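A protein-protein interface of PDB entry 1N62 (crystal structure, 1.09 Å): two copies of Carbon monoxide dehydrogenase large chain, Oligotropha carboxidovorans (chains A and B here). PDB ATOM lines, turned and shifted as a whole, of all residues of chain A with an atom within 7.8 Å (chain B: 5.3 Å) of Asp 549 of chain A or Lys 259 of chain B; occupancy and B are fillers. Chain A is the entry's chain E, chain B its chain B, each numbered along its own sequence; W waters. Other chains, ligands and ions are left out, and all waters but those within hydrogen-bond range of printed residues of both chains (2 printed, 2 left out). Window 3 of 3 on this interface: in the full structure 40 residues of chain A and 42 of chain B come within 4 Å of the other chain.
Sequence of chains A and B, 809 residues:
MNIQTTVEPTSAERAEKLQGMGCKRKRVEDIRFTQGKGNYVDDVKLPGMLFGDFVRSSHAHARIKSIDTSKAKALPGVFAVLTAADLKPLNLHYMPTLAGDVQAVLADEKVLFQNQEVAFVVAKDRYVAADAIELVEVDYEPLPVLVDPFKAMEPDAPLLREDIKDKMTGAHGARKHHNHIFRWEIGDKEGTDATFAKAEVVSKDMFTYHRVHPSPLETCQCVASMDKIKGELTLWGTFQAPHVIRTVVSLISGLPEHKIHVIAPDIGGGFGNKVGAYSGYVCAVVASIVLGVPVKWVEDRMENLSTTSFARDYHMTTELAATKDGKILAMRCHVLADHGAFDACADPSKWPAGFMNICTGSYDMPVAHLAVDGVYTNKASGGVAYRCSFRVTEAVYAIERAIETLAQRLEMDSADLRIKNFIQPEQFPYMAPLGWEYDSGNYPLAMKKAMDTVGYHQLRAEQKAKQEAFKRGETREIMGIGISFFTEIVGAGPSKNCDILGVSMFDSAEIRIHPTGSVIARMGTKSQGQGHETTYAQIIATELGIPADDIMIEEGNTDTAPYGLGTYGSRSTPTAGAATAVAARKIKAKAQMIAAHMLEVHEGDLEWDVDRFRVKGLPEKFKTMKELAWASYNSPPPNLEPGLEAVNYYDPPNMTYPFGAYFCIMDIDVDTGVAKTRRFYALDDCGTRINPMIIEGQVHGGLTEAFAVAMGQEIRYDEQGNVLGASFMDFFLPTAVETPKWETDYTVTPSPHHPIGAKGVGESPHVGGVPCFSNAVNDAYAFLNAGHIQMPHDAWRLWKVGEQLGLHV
ND1 of His 258 of chain B lies within hydrogen-bond range of O of Asp 550 of chain A (3.5 Å).
The backbone carbonyl oxygen (O) of Asp 549 of chain A sits close to a ring nitrogen (NE2) of His 258 of chain B.
OG of Ser 518 of chain A lies within hydrogen-bond range of N of His 258 of chain B (3.3 Å).
OG of Ser 518 of chain A sits at hydrogen-bond distance from N of Glu 257 of chain B (3.4 Å).
Of the 11 printed residues of chain B, 4 touch a printed residue of chain A.
Along chain B the printed residues that touch a printed residue of chain A span positions 232 to 259.
Of the 23 printed residues of chain A, 7 touch a printed residue of chain B.
Printed residues of chain A that touch a printed residue of chain B: His 514, Ser 518, Val 519, Asp 549, Asp 550, Ile 551 and Met 552.
Hydrophobic or aromatic side chains of chain A that line the printed part of chain B: His 514 and Met 552.
Among the printed residues, 11 pairs touch across the chains.
Water W2 lies within hydrogen-bond range of OG of Ser 518 of chain A (2.7 Å) and N of Glu 257 of chain B (2.8 Å).
Water W1 lies within hydrogen-bond range of the side-chain amino group of Lys 259 of chain B and the side-chain carboxylate of Asp 549 of chain A.
The backbone carbonyl oxygen of Lys 259 of chain B is in hydrogen-bond range of the backbone NH of Leu 233 of chain B, at 2.8 Å.
The side-chain carboxylate (OD1) of Asp 549 of chain A is in salt-bridge range of the guanidinium group (NH2) of Arg 25 of chain A (2.8 Å).
O of Asp 550 of chain A is in hydrogen-bond range of N of Val 519 of chain A, at 2.9 Å.
The side-chain carboxylate (OE1) of Glu 232 of chain B sits at hydrogen-bond distance from a ring nitrogen (NE2) of His 261 of chain B (2.7 Å).
O of Val 519 of chain A lies within hydrogen-bond range of N of Met 552 of chain A, 2.8 Å away.
Among the printed residues, merely in contact across the chains: His 514 of chain A with Glu 257 of chain B (3.5 Å), His 514 of chain A with His 258 of chain B (3.8 Å), Val 519 of chain A with His 258 of chain B (3.4 Å), Asp 549 of chain A with Lys 259 of chain B (3.97 Å), Ile 551 of chain A with His 258 of chain B (3.5 Å), Met 552 of chain A with Glu 232 of chain B (3.5 Å) and Met 552 of chain A with His 258 of chain B (3.5 Å).
No position is printed for both chains.
Of the 11 pairs that touch across the chains among the printed residues, none has its exchanged pair printed and touching as well.
Glu 16 of chain A touches none of the printed residues of chain B.
Of the printed residues of chain B, His 514 of chain A touches Glu 257 and His 258.
Of the printed residues of chain B, Ser 518 of chain A touches Glu 257 and His 258.
Of the printed residues of chain B, Val 519 of chain A touches His 258.
Thr 534 of chain A touches none of the printed residues of chain B.
Of chain B, only His 258 (2.8 Å) and Lys 259 (3.97 Å) come within 4 Å of Asp 549 of chain A.
Lys 259 of chain B touches just one residue of chain A: Asp 549.
The nearest printed residue of chain B that does not touch Asp 549 of chain A is Pro 256 of chain B (5.6 Å).
The nearest printed residue of chain B that does not touch Asp 550 of chain A is Pro 256 of chain B (5.4 Å).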
ATOM      1  N   GLU A  16     -17.347   1.376  -7.152  1.00  0.00           N
ATOM      2  CA  GLU A  16     -18.237   0.248  -7.365  1.00  0.00           C
ATOM      3  C   GLU A  16     -18.716  -0.252  -6.013  1.00  0.00           C
ATOM      4  O   GLU A  16     -19.722  -0.951  -5.935  1.00  0.00           O
ATOM      5  N   LYS A  17     -17.797  -0.236  -5.054  1.00  0.00           N
ATOM      6  CA  LYS A  17     -18.008  -0.996  -3.833  1.00  0.00           C
ATOM      7  C   LYS A  17     -18.869  -0.200  -2.849  1.00  0.00           C
ATOM      8  O   LYS A  17     -19.317  -0.727  -1.856  1.00  0.00           O
ATOM      9  CB  LYS A  17     -16.667  -1.428  -3.211  1.00  0.00           C
ATOM     10  N   LEU A  18     -18.994   1.107  -3.024  1.00  0.00           N
ATOM     11  CA  LEU A  18     -19.551   1.891  -1.916  1.00  0.00           C
ATOM     12  C   LEU A  18     -20.996   1.478  -1.587  1.00  0.00           C
ATOM     13  O   LEU A  18     -21.332   1.231  -0.444  1.00  0.00           O
ATOM     14  CB  LEU A  18     -19.487   3.370  -2.202  1.00  0.00           C
ATOM     15  CG  LEU A  18     -19.788   4.209  -0.976  1.00  0.00           C
ATOM     16  CD1 LEU A  18     -18.756   4.028   0.146  1.00  0.00           C
ATOM     17  CD2 LEU A  18     -19.871   5.639  -1.398  1.00  0.00           C
ATOM     18  N   GLN A  19     -21.836   1.445  -2.607  1.00  0.00           N
ATOM     19  CA  GLN A  19     -23.230   1.049  -2.455  1.00  0.00           C
ATOM     20  C   GLN A  19     -23.935   1.793  -1.350  1.00  0.00           C
ATOM     21  O   GLN A  19     -24.637   1.222  -0.507  1.00  0.00           O
ATOM     22  CB  GLN A  19     -23.345  -0.457  -2.260  1.00  0.00           C
ATOM     23  CG  GLN A  19     -22.877  -1.239  -3.455  1.00  0.00           C
ATOM     24  CD  GLN A  19     -23.572  -2.600  -3.573  1.00  0.00           C
ATOM     25  N   GLY A  20     -23.780   3.101  -1.401  1.00  0.00           N
ATOM     26  CA  GLY A  20     -24.366   3.952  -0.411  1.00  0.00           C
ATOM     27  C   GLY A  20     -25.727   4.450  -0.780  1.00  0.00           C
ATOM     28  O   GLY A  20     -26.495   3.792  -1.488  1.00  0.00           O
ATOM     29  N   ARG A  25     -29.020  -1.146  -3.859  1.00  0.00           N
ATOM     30  CA  ARG A  25     -28.177  -2.160  -3.284  1.00  0.00           C
ATOM     31  C   ARG A  25     -29.015  -3.403  -3.098  1.00  0.00           C
ATOM     32  O   ARG A  25     -30.095  -3.360  -2.509  1.00  0.00           O
ATOM     33  CB  ARG A  25     -27.642  -1.689  -1.962  1.00  0.00           C
ATOM     34  CG  ARG A  25     -26.728  -2.653  -1.339  1.00  0.00           C
ATOM     35  CD  ARG A  25     -26.163  -2.244  -0.004  1.00  0.00           C
ATOM     36  NE  ARG A  25     -25.271  -3.275   0.481  1.00  0.00           N
ATOM     37  CZ  ARG A  25     -25.068  -3.595   1.744  1.00  0.00           C
ATOM     38  NH1 ARG A  25     -25.778  -3.059   2.723  1.00  0.00           N
ATOM     39  NH2 ARG A  25     -24.136  -4.474   2.034  1.00  0.00           N
ATOM     40  N   LYS A  26     -28.485  -4.512  -3.559  1.00  0.00           N
ATOM     41  CA  LYS A  26     -29.170  -5.752  -3.398  1.00  0.00           C
ATOM     42  C   LYS A  26     -29.047  -6.172  -1.966  1.00  0.00           C
ATOM     43  O   LYS A  26     -28.120  -5.781  -1.238  1.00  0.00           O
ATOM     44  CB  LYS A  26     -28.626  -6.802  -4.343  1.00  0.00           C
ATOM     45  CG  LYS A  26     -28.702  -6.415  -5.800  1.00  0.00           C
ATOM     46  CD  LYS A  26     -30.143  -6.070  -6.196  1.00  0.00           C
ATOM     47  CE  LYS A  26     -30.237  -5.259  -7.478  1.00  0.00           C
ATOM     48  NZ  LYS A  26     -30.098  -6.083  -8.699  1.00  0.00           N
ATOM     49  N   ARG A  27     -30.046  -6.903  -1.516  1.00  0.00           N
ATOM     50  CA  ARG A  27     -30.193  -7.095  -0.106  1.00  0.00           C
ATOM     51  C   ARG A  27     -29.294  -8.149   0.455  1.00  0.00           C
ATOM     52  O   ARG A  27     -29.219  -9.261  -0.047  1.00  0.00           O
ATOM     53  CB  ARG A  27     -31.616  -7.449   0.242  1.00  0.00           C
ATOM     54  CG  ARG A  27     -32.569  -6.438  -0.174  1.00  0.00           C
ATOM     55  CD  ARG A  27     -33.887  -6.499   0.462  1.00  0.00           C
ATOM     56  NE  ARG A  27     -34.347  -7.857   0.667  1.00  0.00           N
ATOM     57  CZ  ARG A  27     -34.985  -8.218   1.750  1.00  0.00           C
ATOM     58  NH1 ARG A  27     -35.554  -7.337   2.526  1.00  0.00           N
ATOM     59  NH2 ARG A  27     -35.009  -9.466   2.094  1.00  0.00           N
ATOM     60  N   VAL A  28     -28.664  -7.816   1.562  1.00  0.00           N
ATOM     61  CA  VAL A  28     -27.832  -8.773   2.230  1.00  0.00           C
ATOM     62  C   VAL A  28     -28.651  -9.891   2.831  1.00  0.00           C
ATOM     63  O   VAL A  28     -28.152 -10.998   2.918  1.00  0.00           O
ATOM     64  CB  VAL A  28     -26.906  -8.159   3.281  1.00  0.00           C
ATOM     65  CG1 VAL A  28     -25.929  -7.226   2.600  1.00  0.00           C
ATOM     66  CG2 VAL A  28     -27.674  -7.432   4.361  1.00  0.00           C
ATOM     67  N   HIS A 514     -13.984  -0.978  13.274  1.00  0.00           N
ATOM     68  CA  HIS A 514     -12.924  -1.842  13.675  1.00  0.00           C
ATOM     69  C   HIS A 514     -11.591  -1.306  13.182  1.00  0.00           C
ATOM     70  O   HIS A 514     -11.524  -0.475  12.281  1.00  0.00           O
ATOM     71  CB  HIS A 514     -13.200  -3.211  13.072  1.00  0.00           C
ATOM     72  CG  HIS A 514     -14.440  -3.814  13.588  1.00  0.00           C
ATOM     73  ND1 HIS A 514     -14.822  -3.641  14.903  1.00  0.00           N
ATOM     74  CD2 HIS A 514     -15.350  -4.630  13.007  1.00  0.00           C
ATOM     75  CE1 HIS A 514     -15.934  -4.340  15.102  1.00  0.00           C
ATOM     76  NE2 HIS A 514     -16.298  -4.888  13.961  1.00  0.00           N
ATOM     77  N   SER A 518     -13.800  -2.120   8.858  1.00  0.00           N
ATOM     78  CA  SER A 518     -15.145  -2.606   8.774  1.00  0.00           C
ATOM     79  C   SER A 518     -15.890  -2.187  10.008  1.00  0.00           C
ATOM     80  O   SER A 518     -15.308  -1.575  10.926  1.00  0.00           O
ATOM     81  CB  SER A 518     -15.141  -4.108   8.592  1.00  0.00           C
ATOM     82  OG  SER A 518     -14.394  -4.702   9.641  1.00  0.00           O
ATOM     83  N   VAL A 519     -17.179  -2.428  10.016  1.00  0.00           N
ATOM     84  CA  VAL A 519     -18.071  -1.779  10.945  1.00  0.00           C
ATOM     85  C   VAL A 519     -19.113  -2.751  11.445  1.00  0.00           C
ATOM     86  O   VAL A 519     -19.651  -3.522  10.656  1.00  0.00           O
ATOM     87  CB  VAL A 519     -18.783  -0.684  10.231  1.00  0.00           C
ATOM     88  CG1 VAL A 519     -19.713   0.058  11.158  1.00  0.00           C
ATOM     89  CG2 VAL A 519     -17.774   0.241   9.590  1.00  0.00           C
ATOM     90  N   THR A 534     -29.777  -4.037   4.956  1.00  0.00           N
ATOM     91  CA  THR A 534     -29.197  -3.502   3.746  1.00  0.00           C
ATOM     92  C   THR A 534     -29.103  -1.980   3.806  1.00  0.00           C
ATOM     93  O   THR A 534     -28.080  -1.372   3.519  1.00  0.00           O
ATOM     94  CB  THR A 534     -30.020  -3.954   2.574  1.00  0.00           C
ATOM     95  OG1 THR A 534     -29.908  -5.365   2.475  1.00  0.00           O
ATOM     96  CG2 THR A 534     -29.516  -3.426   1.287  1.00  0.00           C
ATOM     97  N   ALA A 537     -26.900   0.296   6.329  1.00  0.00           N
ATOM     98  CA  ALA A 537     -25.510   0.289   5.929  1.00  0.00           C
ATOM     99  C   ALA A 537     -25.278   1.283   4.819  1.00  0.00           C
ATOM    100  O   ALA A 537     -24.192   1.838   4.739  1.00  0.00           O
ATOM    101  CB  ALA A 537     -25.091  -1.057   5.500  1.00  0.00           C
ATOM    102  N   GLN A 538     -26.262   1.516   3.969  1.00  0.00           N
ATOM    103  CA  GLN A 538     -26.105   2.472   2.916  1.00  0.00           C
ATOM    104  C   GLN A 538     -25.985   3.864   3.465  1.00  0.00           C
ATOM    105  O   GLN A 538     -25.224   4.676   2.946  1.00  0.00           O
ATOM    106  CB  GLN A 538     -27.299   2.403   1.971  1.00  0.00           C
ATOM    107  CG  GLN A 538     -27.363   1.099   1.235  1.00  0.00           C
ATOM    108  CD  GLN A 538     -28.518   1.017   0.292  1.00  0.00           C
ATOM    109  OE1 GLN A 538     -29.488   0.283   0.551  1.00  0.00           O
ATOM    110  NE2 GLN A 538     -28.466   1.748  -0.781  1.00  0.00           N
ATOM    111  N   ALA A 541     -22.473   4.041   4.813  1.00  0.00           N
ATOM    112  CA  ALA A 541     -21.544   4.029   3.703  1.00  0.00           C
ATOM    113  C   ALA A 541     -21.338   5.408   3.133  1.00  0.00           C
ATOM    114  O   ALA A 541     -20.218   5.847   2.909  1.00  0.00           O
ATOM    115  CB  ALA A 541     -21.994   3.071   2.651  1.00  0.00           C
ATOM    116  N   ILE A 546     -17.328   4.232   3.657  1.00  0.00           N
ATOM    117  CA  ILE A 546     -16.993   2.848   3.934  1.00  0.00           C
ATOM    118  C   ILE A 546     -17.947   2.011   3.101  1.00  0.00           C
ATOM    119  O   ILE A 546     -19.143   2.179   3.211  1.00  0.00           O
ATOM    120  CB  ILE A 546     -17.148   2.540   5.406  1.00  0.00           C
ATOM    121  CG1 ILE A 546     -16.090   3.324   6.202  1.00  0.00           C
ATOM    122  CG2 ILE A 546     -17.032   1.058   5.653  1.00  0.00           C
ATOM    123  CD1 ILE A 546     -16.237   3.188   7.684  1.00  0.00           C
ATOM    124  N   PRO A 547     -17.452   1.099   2.284  1.00  0.00           N
ATOM    125  CA  PRO A 547     -18.349   0.276   1.470  1.00  0.00           C
ATOM    126  C   PRO A 547     -19.421  -0.330   2.340  1.00  0.00           C
ATOM    127  O   PRO A 547     -19.160  -0.883   3.397  1.00  0.00           O
ATOM    128  CB  PRO A 547     -17.420  -0.783   0.883  1.00  0.00           C
ATOM    129  CG  PRO A 547     -16.110  -0.128   0.838  1.00  0.00           C
ATOM    130  CD  PRO A 547     -16.038   0.807   2.024  1.00  0.00           C
ATOM    131  N   ALA A 548     -20.622  -0.439   1.797  1.00  0.00           N
ATOM    132  CA  ALA A 548     -21.724  -0.972   2.568  1.00  0.00           C
ATOM    133  C   ALA A 548     -21.456  -2.393   2.961  1.00  0.00           C
ATOM    134  O   ALA A 548     -21.880  -2.806   4.007  1.00  0.00           O
ATOM    135  CB  ALA A 548     -23.015  -0.862   1.764  1.00  0.00           C
ATOM    136  N   ASP A 549     -20.787  -3.157   2.113  1.00  0.00           N
ATOM    137  CA  ASP A 549     -20.529  -4.537   2.473  1.00  0.00           C
ATOM    138  C   ASP A 549     -19.516  -4.672   3.581  1.00  0.00           C
ATOM    139  O   ASP A 549     -19.350  -5.761   4.102  1.00  0.00           O
ATOM    140  CB  ASP A 549     -20.061  -5.345   1.284  1.00  0.00           C
ATOM    141  CG  ASP A 549     -21.176  -5.647   0.373  1.00  0.00           C
ATOM    142  OD1 ASP A 549     -22.231  -6.151   0.858  1.00  0.00           O
ATOM    143  OD2 ASP A 549     -21.093  -5.368  -0.829  1.00  0.00           O
ATOM    144  N   ASP A 550     -18.826  -3.588   3.921  1.00  0.00           N
ATOM    145  CA  ASP A 550     -17.914  -3.615   5.040  1.00  0.00           C
ATOM    146  C   ASP A 550     -18.623  -3.271   6.335  1.00  0.00           C
ATOM    147  O   ASP A 550     -17.969  -3.089   7.347  1.00  0.00           O
ATOM    148  CB  ASP A 550     -16.784  -2.631   4.856  1.00  0.00           C
ATOM    149  CG  ASP A 550     -15.903  -2.961   3.715  1.00  0.00           C
ATOM    150  OD1 ASP A 550     -16.027  -4.053   3.136  1.00  0.00           O
ATOM    151  OD2 ASP A 550     -14.971  -2.196   3.399  1.00  0.00           O
ATOM    152  N   ILE A 551     -19.943  -3.247   6.316  1.00  0.00           N
ATOM    153  CA  ILE A 551     -20.721  -2.820   7.460  1.00  0.00           C
ATOM    154  C   ILE A 551     -21.711  -3.910   7.754  1.00  0.00           C
ATOM    155  O   ILE A 551     -22.461  -4.302   6.880  1.00  0.00           O
ATOM    156  CB  ILE A 551     -21.472  -1.522   7.113  1.00  0.00           C
ATOM    157  CG1 ILE A 551     -20.467  -0.438   6.728  1.00  0.00           C
ATOM    158  CG2 ILE A 551     -22.327  -1.064   8.268  1.00  0.00           C
ATOM    159  CD1 ILE A 551     -21.089   0.792   6.159  1.00  0.00           C
ATOM    160  N   MET A 552     -21.770  -4.326   8.999  1.00  0.00           N
ATOM    161  CA  MET A 552     -22.737  -5.296   9.461  1.00  0.00           C
ATOM    162  C   MET A 552     -23.779  -4.586  10.261  1.00  0.00           C
ATOM    163  O   MET A 552     -23.429  -3.859  11.161  1.00  0.00           O
ATOM    164  CB  MET A 552     -22.050  -6.314  10.365  1.00  0.00           C
ATOM    165  CG  MET A 552     -23.007  -7.320  10.923  1.00  0.00           C
ATOM    166  SD  MET A 552     -23.627  -8.403   9.664  1.00  0.00           S
ATOM    167  CE  MET A 552     -22.100  -9.130   9.086  1.00  0.00           C
ATOM    168  N   LYS B 230     -23.134 -17.440   4.647  1.00  0.00           N
ATOM    169  CA  LYS B 230     -23.039 -16.017   4.951  1.00  0.00           C
ATOM    170  C   LYS B 230     -21.681 -15.393   4.714  1.00  0.00           C
ATOM    171  O   LYS B 230     -21.524 -14.177   4.753  1.00  0.00           O
ATOM    172  CB  LYS B 230     -23.422 -15.799   6.388  1.00  0.00           C
ATOM    173  CG  LYS B 230     -24.803 -16.263   6.677  1.00  0.00           C
ATOM    174  CD  LYS B 230     -25.127 -16.028   8.099  1.00  0.00           C
ATOM    175  CE  LYS B 230     -26.506 -16.475   8.419  1.00  0.00           C
ATOM    176  NZ  LYS B 230     -26.808 -16.226   9.837  1.00  0.00           N
ATOM    177  N   GLY B 231     -20.658 -16.211   4.577  1.00  0.00           N
ATOM    178  CA  GLY B 231     -19.306 -15.691   4.528  1.00  0.00           C
ATOM    179  C   GLY B 231     -18.831 -15.122   5.837  1.00  0.00           C
ATOM    180  O   GLY B 231     -18.074 -14.174   5.860  1.00  0.00           O
ATOM    181  N   GLU B 232     -19.239 -15.729   6.929  1.00  0.00           N
ATOM    182  CA  GLU B 232     -18.895 -15.236   8.248  1.00  0.00           C
ATOM    183  C   GLU B 232     -18.313 -16.321   9.092  1.00  0.00           C
ATOM    184  O   GLU B 232     -18.829 -17.436   9.118  1.00  0.00           O
ATOM    185  CB  GLU B 232     -20.109 -14.733   8.982  1.00  0.00           C
ATOM    186  CG  GLU B 232     -20.723 -13.562   8.275  1.00  0.00           C
ATOM    187  CD  GLU B 232     -21.991 -13.089   8.909  1.00  0.00           C
ATOM    188  OE1 GLU B 232     -22.124 -13.216  10.141  1.00  0.00           O
ATOM    189  OE2 GLU B 232     -22.800 -12.482   8.177  1.00  0.00           O
ATOM    190  N   LEU B 233     -17.224 -16.015   9.743  1.00  0.00           N
ATOM    191  CA  LEU B 233     -16.533 -16.937  10.586  1.00  0.00           C
ATOM    192  C   LEU B 233     -16.883 -16.660  12.019  1.00  0.00           C
ATOM    193  O   LEU B 233     -16.726 -15.545  12.486  1.00  0.00           O
ATOM    194  CB  LEU B 233     -15.033 -16.751  10.390  1.00  0.00           C
ATOM    195  CG  LEU B 233     -14.173 -17.565  11.314  1.00  0.00           C
ATOM    196  CD1 LEU B 233     -14.323 -19.010  11.010  1.00  0.00           C
ATOM    197  CD2 LEU B 233     -12.708 -17.133  11.172  1.00  0.00           C
ATOM    198  N   LEU B 255     -10.716 -12.267   5.716  1.00  0.00           N
ATOM    199  CA  LEU B 255     -12.101 -11.958   6.051  1.00  0.00           C
ATOM    200  C   LEU B 255     -12.059 -10.684   6.818  1.00  0.00           C
ATOM    201  O   LEU B 255     -11.215 -10.478   7.666  1.00  0.00           O
ATOM    202  CB  LEU B 255     -12.725 -13.047   6.916  1.00  0.00           C
ATOM    203  CG  LEU B 255     -12.902 -14.379   6.226  1.00  0.00           C
ATOM    204  CD1 LEU B 255     -13.201 -15.443   7.250  1.00  0.00           C
ATOM    205  CD2 LEU B 255     -14.008 -14.270   5.210  1.00  0.00           C
ATOM    206  N   PRO B 256     -13.056  -9.870   6.605  1.00  0.00           N
ATOM    207  CA  PRO B 256     -13.150  -8.599   7.308  1.00  0.00           C
ATOM    208  C   PRO B 256     -13.647  -8.808   8.709  1.00  0.00           C
ATOM    209  O   PRO B 256     -14.324  -9.784   8.989  1.00  0.00           O
ATOM    210  CB  PRO B 256     -14.128  -7.830   6.471  1.00  0.00           C
ATOM    211  CG  PRO B 256     -15.064  -8.905   5.929  1.00  0.00           C
ATOM    212  CD  PRO B 256     -14.141 -10.048   5.624  1.00  0.00           C
ATOM    213  N   GLU B 257     -13.246  -7.914   9.595  1.00  0.00           N
ATOM    214  CA  GLU B 257     -13.491  -8.075  10.996  1.00  0.00           C
ATOM    215  C   GLU B 257     -14.954  -8.148  11.356  1.00  0.00           C
ATOM    216  O   GLU B 257     -15.324  -8.800  12.326  1.00  0.00           O
ATOM    217  CB  GLU B 257     -12.810  -6.982  11.760  1.00  0.00           C
ATOM    218  CG  GLU B 257     -11.315  -7.156  11.875  1.00  0.00           C
ATOM    219  CD  GLU B 257     -10.713  -6.144  12.807  1.00  0.00           C
ATOM    220  OE1 GLU B 257     -10.746  -6.415  14.015  1.00  0.00           O
ATOM    221  OE2 GLU B 257     -10.316  -5.059  12.341  1.00  0.00           O
ATOM    222  N   HIS B 258     -15.816  -7.473  10.605  1.00  0.00           N
ATOM    223  CA  HIS B 258     -17.231  -7.534  10.931  1.00  0.00           C
ATOM    224  C   HIS B 258     -17.849  -8.854  10.530  1.00  0.00           C
ATOM    225  O   HIS B 258     -18.974  -9.128  10.930  1.00  0.00           O
ATOM    226  CB  HIS B 258     -18.027  -6.441  10.253  1.00  0.00           C
ATOM    227  CG  HIS B 258     -17.973  -6.532   8.781  1.00  0.00           C
ATOM    228  ND1 HIS B 258     -19.049  -6.313   7.941  1.00  0.00           N
ATOM    229  CD2 HIS B 258     -16.902  -6.718   7.997  1.00  0.00           C
ATOM    230  CE1 HIS B 258     -18.640  -6.476   6.694  1.00  0.00           C
ATOM    231  NE2 HIS B 258     -17.339  -6.700   6.706  1.00  0.00           N
ATOM    232  N   LYS B 259     -17.094  -9.705   9.855  1.00  0.00           N
ATOM    233  CA  LYS B 259     -17.559 -11.024   9.497  1.00  0.00           C
ATOM    234  C   LYS B 259     -16.792 -12.067  10.238  1.00  0.00           C
ATOM    235  O   LYS B 259     -16.837 -13.199   9.858  1.00  0.00           O
ATOM    236  CB  LYS B 259     -17.540 -11.216   7.976  1.00  0.00           C
ATOM    237  CG  LYS B 259     -18.513 -10.287   7.340  1.00  0.00           C
ATOM    238  CD  LYS B 259     -18.724 -10.470   5.894  1.00  0.00           C
ATOM    239  CE  LYS B 259     -19.873  -9.618   5.392  1.00  0.00           C
ATOM    240  NZ  LYS B 259     -19.965  -9.682   3.918  1.00  0.00           N
ATOM    241  N   ILE B 260     -16.090 -11.674  11.282  1.00  0.00           N
ATOM    242  CA  ILE B 260     -15.389 -12.598  12.151  1.00  0.00           C
ATOM    243  C   ILE B 260     -15.896 -12.342  13.543  1.00  0.00           C
ATOM    244  O   ILE B 260     -15.692 -11.293  14.121  1.00  0.00           O
ATOM    245  CB  ILE B 260     -13.881 -12.405  12.118  1.00  0.00           C
ATOM    246  CG1 ILE B 260     -13.344 -12.603  10.723  1.00  0.00           C
ATOM    247  CG2 ILE B 260     -13.232 -13.401  13.046  1.00  0.00           C
ATOM    248  CD1 ILE B 260     -11.913 -12.115  10.591  1.00  0.00           C
ATOM    249  N   HIS B 261     -16.577 -13.338  14.074  1.00  0.00           N
ATOM    250  CA  HIS B 261     -17.231 -13.246  15.357  1.00  0.00           C
ATOM    251  C   HIS B 261     -16.425 -14.093  16.288  1.00  0.00           C
ATOM    252  O   HIS B 261     -16.605 -15.281  16.333  1.00  0.00           O
ATOM    253  CB  HIS B 261     -18.653 -13.757  15.255  1.00  0.00           C
ATOM    254  CG  HIS B 261     -19.354 -13.201  14.069  1.00  0.00           C
ATOM    255  ND1 HIS B 261     -19.508 -11.855  13.846  1.00  0.00           N
ATOM    256  CD2 HIS B 261     -19.893 -13.823  12.999  1.00  0.00           C
ATOM    257  CE1 HIS B 261     -20.098 -11.677  12.684  1.00  0.00           C
ATOM    258  NE2 HIS B 261     -20.360 -12.857  12.155  1.00  0.00           N
HETATM  259  O   HOH W   1     -22.013  -7.837   3.429  1.00  0.00           O
HETATM  260  O   HOH W   2     -12.187  -5.562   8.392  1.00  0.00           O
